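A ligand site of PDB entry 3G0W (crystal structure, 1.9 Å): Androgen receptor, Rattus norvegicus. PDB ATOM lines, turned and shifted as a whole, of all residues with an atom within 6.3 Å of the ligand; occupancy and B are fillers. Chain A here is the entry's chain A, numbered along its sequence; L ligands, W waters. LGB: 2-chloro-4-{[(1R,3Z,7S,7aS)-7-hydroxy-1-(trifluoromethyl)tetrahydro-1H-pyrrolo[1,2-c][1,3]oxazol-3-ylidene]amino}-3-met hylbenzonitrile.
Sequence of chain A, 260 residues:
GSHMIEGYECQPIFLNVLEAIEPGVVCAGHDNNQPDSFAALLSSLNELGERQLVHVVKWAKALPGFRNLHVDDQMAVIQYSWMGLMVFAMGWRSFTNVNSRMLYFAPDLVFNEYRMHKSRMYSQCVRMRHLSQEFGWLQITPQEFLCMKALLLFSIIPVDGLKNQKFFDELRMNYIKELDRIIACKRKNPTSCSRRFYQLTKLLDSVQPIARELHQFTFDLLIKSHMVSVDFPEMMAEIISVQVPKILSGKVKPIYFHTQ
Water W1 lies within hydrogen-bond range of the guanidinium group of Arg 93 (2.9 Å), the backbone carbonyl oxygen of Met 86 (3.0 Å) and a nitrogen (N20) of the ligand (3.3 Å).
The side-chain amide oxygen (OD1) of Asn 46 lies within hydrogen-bond range of an oxygen (O18) of the ligand, at 2.8 Å.
A nitrogen (N20) of the ligand lies within hydrogen-bond range of the guanidinium group (NH1) of Arg 93 (2.8 Å).
The side-chain hydroxyl of Thr 218 sits close to a nitrogen (N2) of the ligand (3.1 Å).
SD of Met 236 sits close to F24 of the ligand (3.6 Å).
CD1 of Leu 42 touches C5 of the ligand, at 3.6 Å.
Leu 45 touches the ligand.
CD2 of Leu 48 touches C19 of the ligand, 3.7 Å away.
Gly 49 touches the ligand (CA to F24, 3.6 Å).
Gln 52 touches the ligand (CG to N20, 3.7 Å).
Trp 82 touches the ligand (CH2 to F23, 3.2 Å).
CE of Met 83 touches F23 of the ligand, at 3.4 Å.
Met 86 touches the ligand.
N of Val 87 touches CL17 of the ligand (3.97 Å).
Met 90 touches the ligand (CB to CL17, 3.4 Å).
Phe 105 touches the ligand (O to N20, 3.6 Å).
CE of Met 121 touches C1 of the ligand, 3.6 Å away.
Leu 214 touches the ligand (CD1 to C16, 3.7 Å).
Phe 217 touches the ligand.
Leu 221 touches the ligand.
CZ of Phe 232 touches O18 of the ligand (3.7 Å).
Ile 240 touches the ligand (CD1 to F22, 3.6 Å).
Hydrophobic or aromatic side chains that line the ligand: Leu 42, Leu 45, Leu 48, Trp 82, Met 83, Met 86, Met 90, Phe 105, Met 121, Leu 214, Phe 217, Leu 221, Phe 232, Met 236 and Ile 240.
21 residues have an atom within 4 Å of the ligand: Leu 42, Leu 45, Asn 46, Leu 48, Gly 49, Gln 52, Trp 82, Met 83, Met 86, Val 87, Met 90, Arg 93, Phe 105, Met 121, Leu 214, Phe 217, Thr 218, Leu 221, Phe 232, Met 236 and Ile 240.
The nearest printed residue that does not touch the ligand is Met 128 (4.2 Å).
The backbone carbonyl oxygen of Phe 105 lies within hydrogen-bond range of the guanidinium group of Arg 93, 2.9 Å away.
The guanidinium group of Arg 93 lies within hydrogen-bond range of the backbone carbonyl oxygen of Tyr 104.
O of Leu 214 sits at hydrogen-bond distance from OG1 of Thr 218.
The indole nitrogen of Trp 82 is in hydrogen-bond range of the side-chain sulfur of Met 86 (3.3 Å).
O of Gly 49 lies within hydrogen-bond range of NE1 of Trp 82, at 3.5 Å.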
ATOM      1  N   LEU A  42      -5.787  -7.969  18.680  1.00  0.00           N
ATOM      2  CA  LEU A  42      -6.724  -8.516  19.639  1.00  0.00           C
ATOM      3  C   LEU A  42      -6.777  -7.650  20.903  1.00  0.00           C
ATOM      4  O   LEU A  42      -7.849  -7.378  21.424  1.00  0.00           O
ATOM      5  CB  LEU A  42      -6.395  -9.981  19.952  1.00  0.00           C
ATOM      6  CG  LEU A  42      -7.150 -11.017  19.097  1.00  0.00           C
ATOM      7  CD1 LEU A  42      -8.637 -11.056  19.460  1.00  0.00           C
ATOM      8  CD2 LEU A  42      -6.961 -10.779  17.581  1.00  0.00           C
ATOM      9  N   SER A  44      -6.510  -4.557  20.912  1.00  0.00           N
ATOM     10  CA  SER A  44      -7.330  -3.421  20.504  1.00  0.00           C
ATOM     11  C   SER A  44      -8.815  -3.775  20.414  1.00  0.00           C
ATOM     12  O   SER A  44      -9.679  -2.949  20.706  1.00  0.00           O
ATOM     13  CB  SER A  44      -6.824  -2.845  19.177  1.00  0.00           C
ATOM     14  OG  SER A  44      -5.707  -1.994  19.396  1.00  0.00           O
ATOM     15  N   LEU A  45      -9.127  -5.000  20.007  1.00  0.00           N
ATOM     16  CA  LEU A  45     -10.529  -5.434  19.962  1.00  0.00           C
ATOM     17  C   LEU A  45     -11.041  -5.511  21.407  1.00  0.00           C
ATOM     18  O   LEU A  45     -12.174  -5.159  21.686  1.00  0.00           O
ATOM     19  CB  LEU A  45     -10.679  -6.790  19.268  1.00  0.00           C
ATOM     20  CG  LEU A  45     -10.670  -6.746  17.718  1.00  0.00           C
ATOM     21  CD1 LEU A  45     -10.550  -8.143  17.082  1.00  0.00           C
ATOM     22  CD2 LEU A  45     -11.881  -6.009  17.155  1.00  0.00           C
ATOM     23  N   ASN A  46     -10.181  -5.936  22.321  1.00  0.00           N
ATOM     24  CA  ASN A  46     -10.553  -6.029  23.739  1.00  0.00           C
ATOM     25  C   ASN A  46     -10.865  -4.663  24.325  1.00  0.00           C
ATOM     26  O   ASN A  46     -11.899  -4.471  24.964  1.00  0.00           O
ATOM     27  CB  ASN A  46      -9.451  -6.725  24.532  1.00  0.00           C
ATOM     28  CG  ASN A  46      -9.375  -8.196  24.205  1.00  0.00           C
ATOM     29  OD1 ASN A  46     -10.312  -8.743  23.606  1.00  0.00           O
ATOM     30  ND2 ASN A  46      -8.289  -8.837  24.597  1.00  0.00           N
ATOM     31  N   GLU A  47     -10.032  -3.688  24.014  1.00  0.00           N
ATOM     32  CA  GLU A  47     -10.235  -2.329  24.491  1.00  0.00           C
ATOM     33  C   GLU A  47     -11.512  -1.735  23.872  1.00  0.00           C
ATOM     34  O   GLU A  47     -12.318  -1.128  24.570  1.00  0.00           O
ATOM     35  CB  GLU A  47      -9.020  -1.459  24.166  1.00  0.00           C
ATOM     36  CG  GLU A  47      -9.262   0.008  24.468  1.00  0.00           C
ATOM     37  CD  GLU A  47      -9.446   0.257  25.954  1.00  0.00           C
ATOM     38  OE1 GLU A  47     -10.136   1.225  26.323  1.00  0.00           O
ATOM     39  OE2 GLU A  47      -8.922  -0.540  26.755  1.00  0.00           O
ATOM     40  N   LEU A  48     -11.676  -1.914  22.574  1.00  0.00           N
ATOM     41  CA  LEU A  48     -12.862  -1.434  21.872  1.00  0.00           C
ATOM     42  C   LEU A  48     -14.094  -2.144  22.430  1.00  0.00           C
ATOM     43  O   LEU A  48     -15.145  -1.537  22.610  1.00  0.00           O
ATOM     44  CB  LEU A  48     -12.749  -1.712  20.371  1.00  0.00           C
ATOM     45  CG  LEU A  48     -13.968  -1.285  19.566  1.00  0.00           C
ATOM     46  CD1 LEU A  48     -14.205   0.201  19.769  1.00  0.00           C
ATOM     47  CD2 LEU A  48     -13.781  -1.636  18.101  1.00  0.00           C
ATOM     48  N   GLY A  49     -13.960  -3.435  22.685  1.00  0.00           N
ATOM     49  CA  GLY A  49     -15.067  -4.208  23.199  1.00  0.00           C
ATOM     50  C   GLY A  49     -15.545  -3.618  24.510  1.00  0.00           C
ATOM     51  O   GLY A  49     -16.755  -3.516  24.754  1.00  0.00           O
ATOM     52  N   GLU A  50     -14.591  -3.203  25.346  1.00  0.00           N
ATOM     53  CA  GLU A  50     -14.927  -2.608  26.623  1.00  0.00           C
ATOM     54  C   GLU A  50     -15.597  -1.249  26.458  1.00  0.00           C
ATOM     55  O   GLU A  50     -16.628  -0.994  27.055  1.00  0.00           O
ATOM     56  CB  GLU A  50     -13.701  -2.471  27.532  1.00  0.00           C
ATOM     57  CG  GLU A  50     -14.044  -1.773  28.829  1.00  0.00           C
ATOM     58  CD  GLU A  50     -13.130  -2.178  29.956  1.00  0.00           C
ATOM     59  OE1 GLU A  50     -13.079  -3.384  30.293  1.00  0.00           O
ATOM     60  OE2 GLU A  50     -12.455  -1.298  30.510  1.00  0.00           O
ATOM     61  N   GLN A  52     -17.336  -0.238  23.986  1.00  0.00           N
ATOM     62  CA  GLN A  52     -18.678  -0.446  23.441  1.00  0.00           C
ATOM     63  C   GLN A  52     -19.650  -0.915  24.524  1.00  0.00           C
ATOM     64  O   GLN A  52     -20.795  -0.493  24.539  1.00  0.00           O
ATOM     65  CB  GLN A  52     -18.705  -1.443  22.283  1.00  0.00           C
ATOM     66  CG  GLN A  52     -18.095  -0.932  20.968  1.00  0.00           C
ATOM     67  CD  GLN A  52     -18.955   0.090  20.271  1.00  0.00           C
ATOM     68  OE1 GLN A  52     -18.587   0.597  19.221  1.00  0.00           O
ATOM     69  NE2 GLN A  52     -20.132   0.356  20.823  1.00  0.00           N
ATOM     70  N   TRP A  82     -24.650  -8.354  24.802  1.00  0.00           N
ATOM     71  CA  TRP A  82     -23.560  -7.469  24.377  1.00  0.00           C
ATOM     72  C   TRP A  82     -22.835  -7.828  23.064  1.00  0.00           C
ATOM     73  O   TRP A  82     -22.735  -7.005  22.147  1.00  0.00           O
ATOM     74  CB  TRP A  82     -22.607  -7.272  25.548  1.00  0.00           C
ATOM     75  CG  TRP A  82     -21.259  -6.834  25.211  1.00  0.00           C
ATOM     76  CD1 TRP A  82     -20.891  -5.636  24.692  1.00  0.00           C
ATOM     77  CD2 TRP A  82     -20.056  -7.541  25.503  1.00  0.00           C
ATOM     78  NE1 TRP A  82     -19.518  -5.577  24.579  1.00  0.00           N
ATOM     79  CE2 TRP A  82     -18.989  -6.735  25.076  1.00  0.00           C
ATOM     80  CE3 TRP A  82     -19.777  -8.804  26.051  1.00  0.00           C
ATOM     81  CZ2 TRP A  82     -17.649  -7.133  25.175  1.00  0.00           C
ATOM     82  CZ3 TRP A  82     -18.457  -9.208  26.141  1.00  0.00           C
ATOM     83  CH2 TRP A  82     -17.402  -8.363  25.727  1.00  0.00           C
ATOM     84  N   MET A  83     -22.301  -9.036  22.964  1.00  0.00           N
ATOM     85  CA  MET A  83     -21.585  -9.435  21.757  1.00  0.00           C
ATOM     86  C   MET A  83     -22.431  -9.329  20.483  1.00  0.00           C
ATOM     87  O   MET A  83     -21.985  -8.790  19.455  1.00  0.00           O
ATOM     88  CB  MET A  83     -21.024 -10.854  21.931  1.00  0.00           C
ATOM     89  CG  MET A  83     -20.214 -11.394  20.749  1.00  0.00           C
ATOM     90  SD  MET A  83     -18.695 -10.444  20.415  1.00  0.00           S
ATOM     91  CE  MET A  83     -17.688 -10.940  21.787  1.00  0.00           C
ATOM     92  N   MET A  86     -23.047  -5.747  19.490  1.00  0.00           N
ATOM     93  CA  MET A  86     -21.821  -5.173  18.918  1.00  0.00           C
ATOM     94  C   MET A  86     -21.674  -5.637  17.485  1.00  0.00           C
ATOM     95  O   MET A  86     -21.397  -4.839  16.566  1.00  0.00           O
ATOM     96  CB  MET A  86     -20.592  -5.639  19.724  1.00  0.00           C
ATOM     97  CG  MET A  86     -20.235  -4.779  20.954  1.00  0.00           C
ATOM     98  SD  MET A  86     -18.486  -5.002  21.532  1.00  0.00           S
ATOM     99  CE  MET A  86     -18.232  -6.767  21.510  1.00  0.00           C
ATOM    100  N   VAL A  87     -21.899  -6.935  17.273  1.00  0.00           N
ATOM    101  CA  VAL A  87     -21.763  -7.512  15.953  1.00  0.00           C
ATOM    102  C   VAL A  87     -22.700  -6.873  14.944  1.00  0.00           C
ATOM    103  O   VAL A  87     -22.291  -6.522  13.835  1.00  0.00           O
ATOM    104  CB  VAL A  87     -21.923  -9.044  15.992  1.00  0.00           C
ATOM    105  CG1 VAL A  87     -22.104  -9.583  14.587  1.00  0.00           C
ATOM    106  CG2 VAL A  87     -20.729  -9.679  16.659  1.00  0.00           C
ATOM    107  N   PHE A  88     -23.955  -6.725  15.353  1.00  0.00           N
ATOM    108  CA  PHE A  88     -25.005  -6.172  14.517  1.00  0.00           C
ATOM    109  C   PHE A  88     -24.730  -4.714  14.150  1.00  0.00           C
ATOM    110  O   PHE A  88     -24.831  -4.334  12.992  1.00  0.00           O
ATOM    111  CB  PHE A  88     -26.351  -6.307  15.244  1.00  0.00           C
ATOM    112  CG  PHE A  88     -27.545  -6.113  14.373  1.00  0.00           C
ATOM    113  CD1 PHE A  88     -27.833  -7.019  13.370  1.00  0.00           C
ATOM    114  CD2 PHE A  88     -28.428  -5.046  14.584  1.00  0.00           C
ATOM    115  CE1 PHE A  88     -28.971  -6.871  12.568  1.00  0.00           C
ATOM    116  CE2 PHE A  88     -29.549  -4.882  13.791  1.00  0.00           C
ATOM    117  CZ  PHE A  88     -29.819  -5.795  12.777  1.00  0.00           C
ATOM    118  N   MET A  90     -21.831  -3.292  14.242  1.00  0.00           N
ATOM    119  CA  MET A  90     -20.613  -3.256  13.444  1.00  0.00           C
ATOM    120  C   MET A  90     -20.897  -3.607  11.984  1.00  0.00           C
ATOM    121  O   MET A  90     -20.348  -2.985  11.089  1.00  0.00           O
ATOM    122  CB  MET A  90     -19.511  -4.124  14.046  1.00  0.00           C
ATOM    123  CG  MET A  90     -18.196  -3.935  13.329  1.00  0.00           C
ATOM    124  SD  MET A  90     -17.994  -5.006  11.883  1.00  0.00           S
ATOM    125  CE  MET A  90     -17.860  -6.630  12.694  1.00  0.00           C
ATOM    126  N   GLY A  91     -21.819  -4.552  11.752  1.00  0.00           N
ATOM    127  CA  GLY A  91     -22.222  -4.920  10.414  1.00  0.00           C
ATOM    128  C   GLY A  91     -22.841  -3.742   9.687  1.00  0.00           C
ATOM    129  O   GLY A  91     -22.579  -3.526   8.505  1.00  0.00           O
ATOM    130  N   ARG A  93     -22.396  -0.362  10.391  1.00  0.00           N
ATOM    131  CA  ARG A  93     -21.306   0.612  10.151  1.00  0.00           C
ATOM    132  C   ARG A  93     -20.487   0.198   8.919  1.00  0.00           C
ATOM    133  O   ARG A  93     -20.030   1.037   8.134  1.00  0.00           O
ATOM    134  CB  ARG A  93     -20.310   0.593  11.327  1.00  0.00           C
ATOM    135  CG  ARG A  93     -20.765   1.250  12.605  1.00  0.00           C
ATOM    136  CD  ARG A  93     -19.535   1.676  13.443  1.00  0.00           C
ATOM    137  NE  ARG A  93     -18.850   0.554  14.106  1.00  0.00           N
ATOM    138  CZ  ARG A  93     -19.345  -0.153  15.122  1.00  0.00           C
ATOM    139  NH1 ARG A  93     -18.616  -1.122  15.675  1.00  0.00           N
ATOM    140  NH2 ARG A  93     -20.558   0.090  15.592  1.00  0.00           N
ATOM    141  N   TYR A 104     -15.740  -2.591   9.638  1.00  0.00           N
ATOM    142  CA  TYR A 104     -15.524  -1.282  10.254  1.00  0.00           C
ATOM    143  C   TYR A 104     -15.821  -1.310  11.765  1.00  0.00           C
ATOM    144  O   TYR A 104     -16.850  -0.812  12.212  1.00  0.00           O
ATOM    145  CB  TYR A 104     -16.402  -0.244   9.541  1.00  0.00           C
ATOM    146  CG  TYR A 104     -16.043   1.204   9.781  1.00  0.00           C
ATOM    147  CD1 TYR A 104     -15.439   1.962   8.784  1.00  0.00           C
ATOM    148  CD2 TYR A 104     -16.404   1.852  10.962  1.00  0.00           C
ATOM    149  CE1 TYR A 104     -15.176   3.300   8.957  1.00  0.00           C
ATOM    150  CE2 TYR A 104     -16.129   3.193  11.150  1.00  0.00           C
ATOM    151  CZ  TYR A 104     -15.529   3.919  10.139  1.00  0.00           C
ATOM    152  OH  TYR A 104     -15.281   5.263  10.296  1.00  0.00           O
ATOM    153  N   PHE A 105     -14.907  -1.923  12.515  1.00  0.00           N
ATOM    154  CA  PHE A 105     -15.010  -1.995  13.977  1.00  0.00           C
ATOM    155  C   PHE A 105     -15.063  -0.582  14.570  1.00  0.00           C
ATOM    156  O   PHE A 105     -15.878  -0.261  15.446  1.00  0.00           O
ATOM    157  CB  PHE A 105     -13.825  -2.780  14.559  1.00  0.00           C
ATOM    158  CG  PHE A 105     -13.875  -4.262  14.268  1.00  0.00           C
ATOM    159  CD1 PHE A 105     -13.075  -4.818  13.291  1.00  0.00           C
ATOM    160  CD2 PHE A 105     -14.751  -5.091  14.964  1.00  0.00           C
ATOM    161  CE1 PHE A 105     -13.138  -6.199  13.012  1.00  0.00           C
ATOM    162  CE2 PHE A 105     -14.805  -6.460  14.701  1.00  0.00           C
ATOM    163  CZ  PHE A 105     -14.000  -7.004  13.718  1.00  0.00           C
ATOM    164  N   ALA A 106     -14.153   0.254  14.090  1.00  0.00           N
ATOM    165  CA  ALA A 106     -14.080   1.653  14.512  1.00  0.00           C
ATOM    166  C   ALA A 106     -13.346   2.401  13.430  1.00  0.00           C
ATOM    167  O   ALA A 106     -12.673   1.796  12.589  1.00  0.00           O
ATOM    168  CB  ALA A 106     -13.349   1.787  15.844  1.00  0.00           C
ATOM    169  N   MET A 121      -9.251 -14.926  13.469  1.00  0.00           N
ATOM    170  CA  MET A 121     -10.694 -15.140  13.517  1.00  0.00           C
ATOM    171  C   MET A 121     -11.272 -14.946  12.130  1.00  0.00           C
ATOM    172  O   MET A 121     -12.349 -14.377  11.966  1.00  0.00           O
ATOM    173  CB  MET A 121     -11.416 -14.222  14.515  1.00  0.00           C
ATOM    174  CG  MET A 121     -10.576 -13.259  15.308  1.00  0.00           C
ATOM    175  SD  MET A 121     -11.688 -12.206  16.305  1.00  0.00           S
ATOM    176  CE  MET A 121     -12.740 -13.404  16.956  1.00  0.00           C
ATOM    177  N   MET A 128     -19.288 -12.222   9.622  1.00  0.00           N
ATOM    178  CA  MET A 128     -19.677 -10.855   9.958  1.00  0.00           C
ATOM    179  C   MET A 128     -19.765 -10.009   8.693  1.00  0.00           C
ATOM    180  O   MET A 128     -20.676  -9.189   8.546  1.00  0.00           O
ATOM    181  CB  MET A 128     -18.693 -10.261  10.960  1.00  0.00           C
ATOM    182  CG  MET A 128     -18.884 -10.834  12.364  1.00  0.00           C
ATOM    183  SD  MET A 128     -17.923  -9.919  13.590  1.00  0.00           S
ATOM    184  CE  MET A 128     -16.270 -10.586  13.369  1.00  0.00           C
ATOM    185  N   LEU A 214     -17.992 -16.033  18.253  1.00  0.00           N
ATOM    186  CA  LEU A 214     -17.125 -15.000  18.764  1.00  0.00           C
ATOM    187  C   LEU A 214     -16.916 -15.236  20.267  1.00  0.00           C
ATOM    188  O   LEU A 214     -15.807 -15.050  20.780  1.00  0.00           O
ATOM    189  CB  LEU A 214     -17.723 -13.615  18.486  1.00  0.00           C
ATOM    190  CG  LEU A 214     -17.502 -13.118  17.050  1.00  0.00           C
ATOM    191  CD1 LEU A 214     -18.350 -11.892  16.759  1.00  0.00           C
ATOM    192  CD2 LEU A 214     -16.001 -12.822  16.808  1.00  0.00           C
ATOM    193  N   PHE A 217     -14.426 -18.059  20.774  1.00  0.00           N
ATOM    194  CA  PHE A 217     -13.054 -17.623  20.482  1.00  0.00           C
ATOM    195  C   PHE A 217     -12.523 -16.732  21.596  1.00  0.00           C
ATOM    196  O   PHE A 217     -11.378 -16.879  22.057  1.00  0.00           O
ATOM    197  CB  PHE A 217     -13.014 -16.892  19.131  1.00  0.00           C
ATOM    198  CG  PHE A 217     -11.665 -16.319  18.786  1.00  0.00           C
ATOM    199  CD1 PHE A 217     -11.315 -15.043  19.190  1.00  0.00           C
ATOM    200  CD2 PHE A 217     -10.768 -17.049  18.020  1.00  0.00           C
ATOM    201  CE1 PHE A 217     -10.075 -14.500  18.833  1.00  0.00           C
ATOM    202  CE2 PHE A 217      -9.495 -16.527  17.682  1.00  0.00           C
ATOM    203  CZ  PHE A 217      -9.160 -15.245  18.083  1.00  0.00           C
ATOM    204  N   THR A 218     -13.352 -15.798  22.042  1.00  0.00           N
ATOM    205  CA  THR A 218     -12.952 -14.900  23.128  1.00  0.00           C
ATOM    206  C   THR A 218     -12.634 -15.674  24.404  1.00  0.00           C
ATOM    207  O   THR A 218     -11.660 -15.383  25.086  1.00  0.00           O
ATOM    208  CB  THR A 218     -14.034 -13.832  23.403  1.00  0.00           C
ATOM    209  OG1 THR A 218     -14.201 -13.014  22.243  1.00  0.00           O
ATOM    210  CG2 THR A 218     -13.603 -12.975  24.563  1.00  0.00           C
ATOM    211  N   LEU A 221      -9.371 -17.462  24.052  1.00  0.00           N
ATOM    212  CA  LEU A 221      -8.263 -16.505  24.098  1.00  0.00           C
ATOM    213  C   LEU A 221      -8.006 -16.007  25.519  1.00  0.00           C
ATOM    214  O   LEU A 221      -6.864 -15.878  25.928  1.00  0.00           O
ATOM    215  CB  LEU A 221      -8.527 -15.345  23.125  1.00  0.00           C
ATOM    216  CG  LEU A 221      -7.456 -14.271  22.954  1.00  0.00           C
ATOM    217  CD1 LEU A 221      -6.088 -14.920  22.730  1.00  0.00           C
ATOM    218  CD2 LEU A 221      -7.832 -13.353  21.778  1.00  0.00           C
ATOM    219  N   VAL A 230      -1.836 -11.220  24.876  1.00  0.00           N
ATOM    220  CA  VAL A 230      -3.059 -10.455  24.624  1.00  0.00           C
ATOM    221  C   VAL A 230      -3.534  -9.844  25.928  1.00  0.00           C
ATOM    222  O   VAL A 230      -3.584 -10.495  26.971  1.00  0.00           O
ATOM    223  CB  VAL A 230      -4.159 -11.327  23.959  1.00  0.00           C
ATOM    224  CG1 VAL A 230      -5.506 -10.586  23.964  1.00  0.00           C
ATOM    225  CG2 VAL A 230      -3.759 -11.693  22.539  1.00  0.00           C
ATOM    226  N   PHE A 232      -6.377  -8.250  28.305  1.00  0.00           N
ATOM    227  CA  PHE A 232      -7.813  -8.165  28.574  1.00  0.00           C
ATOM    228  C   PHE A 232      -8.040  -7.204  29.718  1.00  0.00           C
ATOM    229  O   PHE A 232      -7.544  -7.419  30.827  1.00  0.00           O
ATOM    230  CB  PHE A 232      -8.382  -9.524  28.965  1.00  0.00           C
ATOM    231  CG  PHE A 232      -8.766 -10.389  27.795  1.00  0.00           C
ATOM    232  CD1 PHE A 232      -7.846 -11.261  27.238  1.00  0.00           C
ATOM    233  CD2 PHE A 232     -10.047 -10.341  27.270  1.00  0.00           C
ATOM    234  CE1 PHE A 232      -8.200 -12.063  26.171  1.00  0.00           C
ATOM    235  CE2 PHE A 232     -10.389 -11.120  26.175  1.00  0.00           C
ATOM    236  CZ  PHE A 232      -9.475 -12.004  25.639  1.00  0.00           C
ATOM    237  N   MET A 236     -13.509  -6.844  31.128  1.00  0.00           N
ATOM    238  CA  MET A 236     -13.733  -7.878  30.119  1.00  0.00           C
ATOM    239  C   MET A 236     -13.457  -9.244  30.746  1.00  0.00           C
ATOM    240  O   MET A 236     -14.256 -10.163  30.605  1.00  0.00           O
ATOM    241  CB  MET A 236     -12.837  -7.672  28.887  1.00  0.00           C
ATOM    242  CG  MET A 236     -13.129  -6.409  28.117  1.00  0.00           C
ATOM    243  SD  MET A 236     -14.826  -6.382  27.482  1.00  0.00           S
ATOM    244  CE  MET A 236     -15.648  -5.459  28.775  1.00  0.00           C
ATOM    245  N   ILE A 240     -16.296 -12.191  30.673  1.00  0.00           N
ATOM    246  CA  ILE A 240     -16.009 -13.383  29.885  1.00  0.00           C
ATOM    247  C   ILE A 240     -15.894 -14.649  30.728  1.00  0.00           C
ATOM    248  O   ILE A 240     -16.142 -15.755  30.257  1.00  0.00           O
ATOM    249  CB  ILE A 240     -14.744 -13.201  29.042  1.00  0.00           C
ATOM    250  CG1 ILE A 240     -14.946 -12.066  28.040  1.00  0.00           C
ATOM    251  CG2 ILE A 240     -14.365 -14.521  28.342  1.00  0.00           C
ATOM    252  CD1 ILE A 240     -13.628 -11.486  27.549  1.00  0.00           C
HETATM  253  C1  LGB L   1     -13.407 -11.231  19.762  1.00  0.00           C
HETATM  254  N2  LGB L   1     -14.009 -10.332  20.773  1.00  0.00           N
HETATM  255  C3  LGB L   1     -13.071 -10.192  21.893  1.00  0.00           C
HETATM  256  C4  LGB L   1     -11.688 -10.600  21.342  1.00  0.00           C
HETATM  257  C5  LGB L   1     -12.044 -11.692  20.269  1.00  0.00           C
HETATM  258  C6  LGB L   1     -14.345  -8.991  20.496  1.00  0.00           C
HETATM  259  O7  LGB L   1     -14.093  -8.186  21.537  1.00  0.00           O
HETATM  260  C8  LGB L   1     -13.245  -8.781  22.451  1.00  0.00           C
HETATM  261  N9  LGB L   1     -14.852  -8.574  19.321  1.00  0.00           N
HETATM  262  C10 LGB L   1     -15.353  -7.351  19.019  1.00  0.00           C
HETATM  263  C11 LGB L   1     -16.392  -7.285  18.058  1.00  0.00           C
HETATM  264  C12 LGB L   1     -16.896  -6.021  17.749  1.00  0.00           C
HETATM  265  C13 LGB L   1     -16.401  -4.846  18.360  1.00  0.00           C
HETATM  266  C14 LGB L   1     -15.396  -4.911  19.296  1.00  0.00           C
HETATM  267  C15 LGB L   1     -14.877  -6.160  19.629  1.00  0.00           C
HETATM  268  C16 LGB L   1     -16.913  -8.532  17.394  1.00  0.00           C
HETATM  269 CL17 LGB L   1     -18.129  -5.899  16.602  1.00  0.00          CL
HETATM  270  O18 LGB L   1     -10.860 -11.124  22.332  1.00  0.00           O
HETATM  271  C19 LGB L   1     -16.896  -3.568  18.066  1.00  0.00           C
HETATM  272  N20 LGB L   1     -17.389  -2.582  17.737  1.00  0.00           N
HETATM  273  C21 LGB L   1     -14.031  -8.790  23.745  1.00  0.00           C
HETATM  274  F22 LGB L   1     -13.297  -9.404  24.660  1.00  0.00           F
HETATM  275  F23 LGB L   1     -15.214  -9.417  23.639  1.00  0.00           F
HETATM  276  F24 LGB L   1     -14.268  -7.558  24.098  1.00  0.00           F
HETATM  277  O   HOH W   1     -20.600  -2.112  17.538  1.00  0.00           O
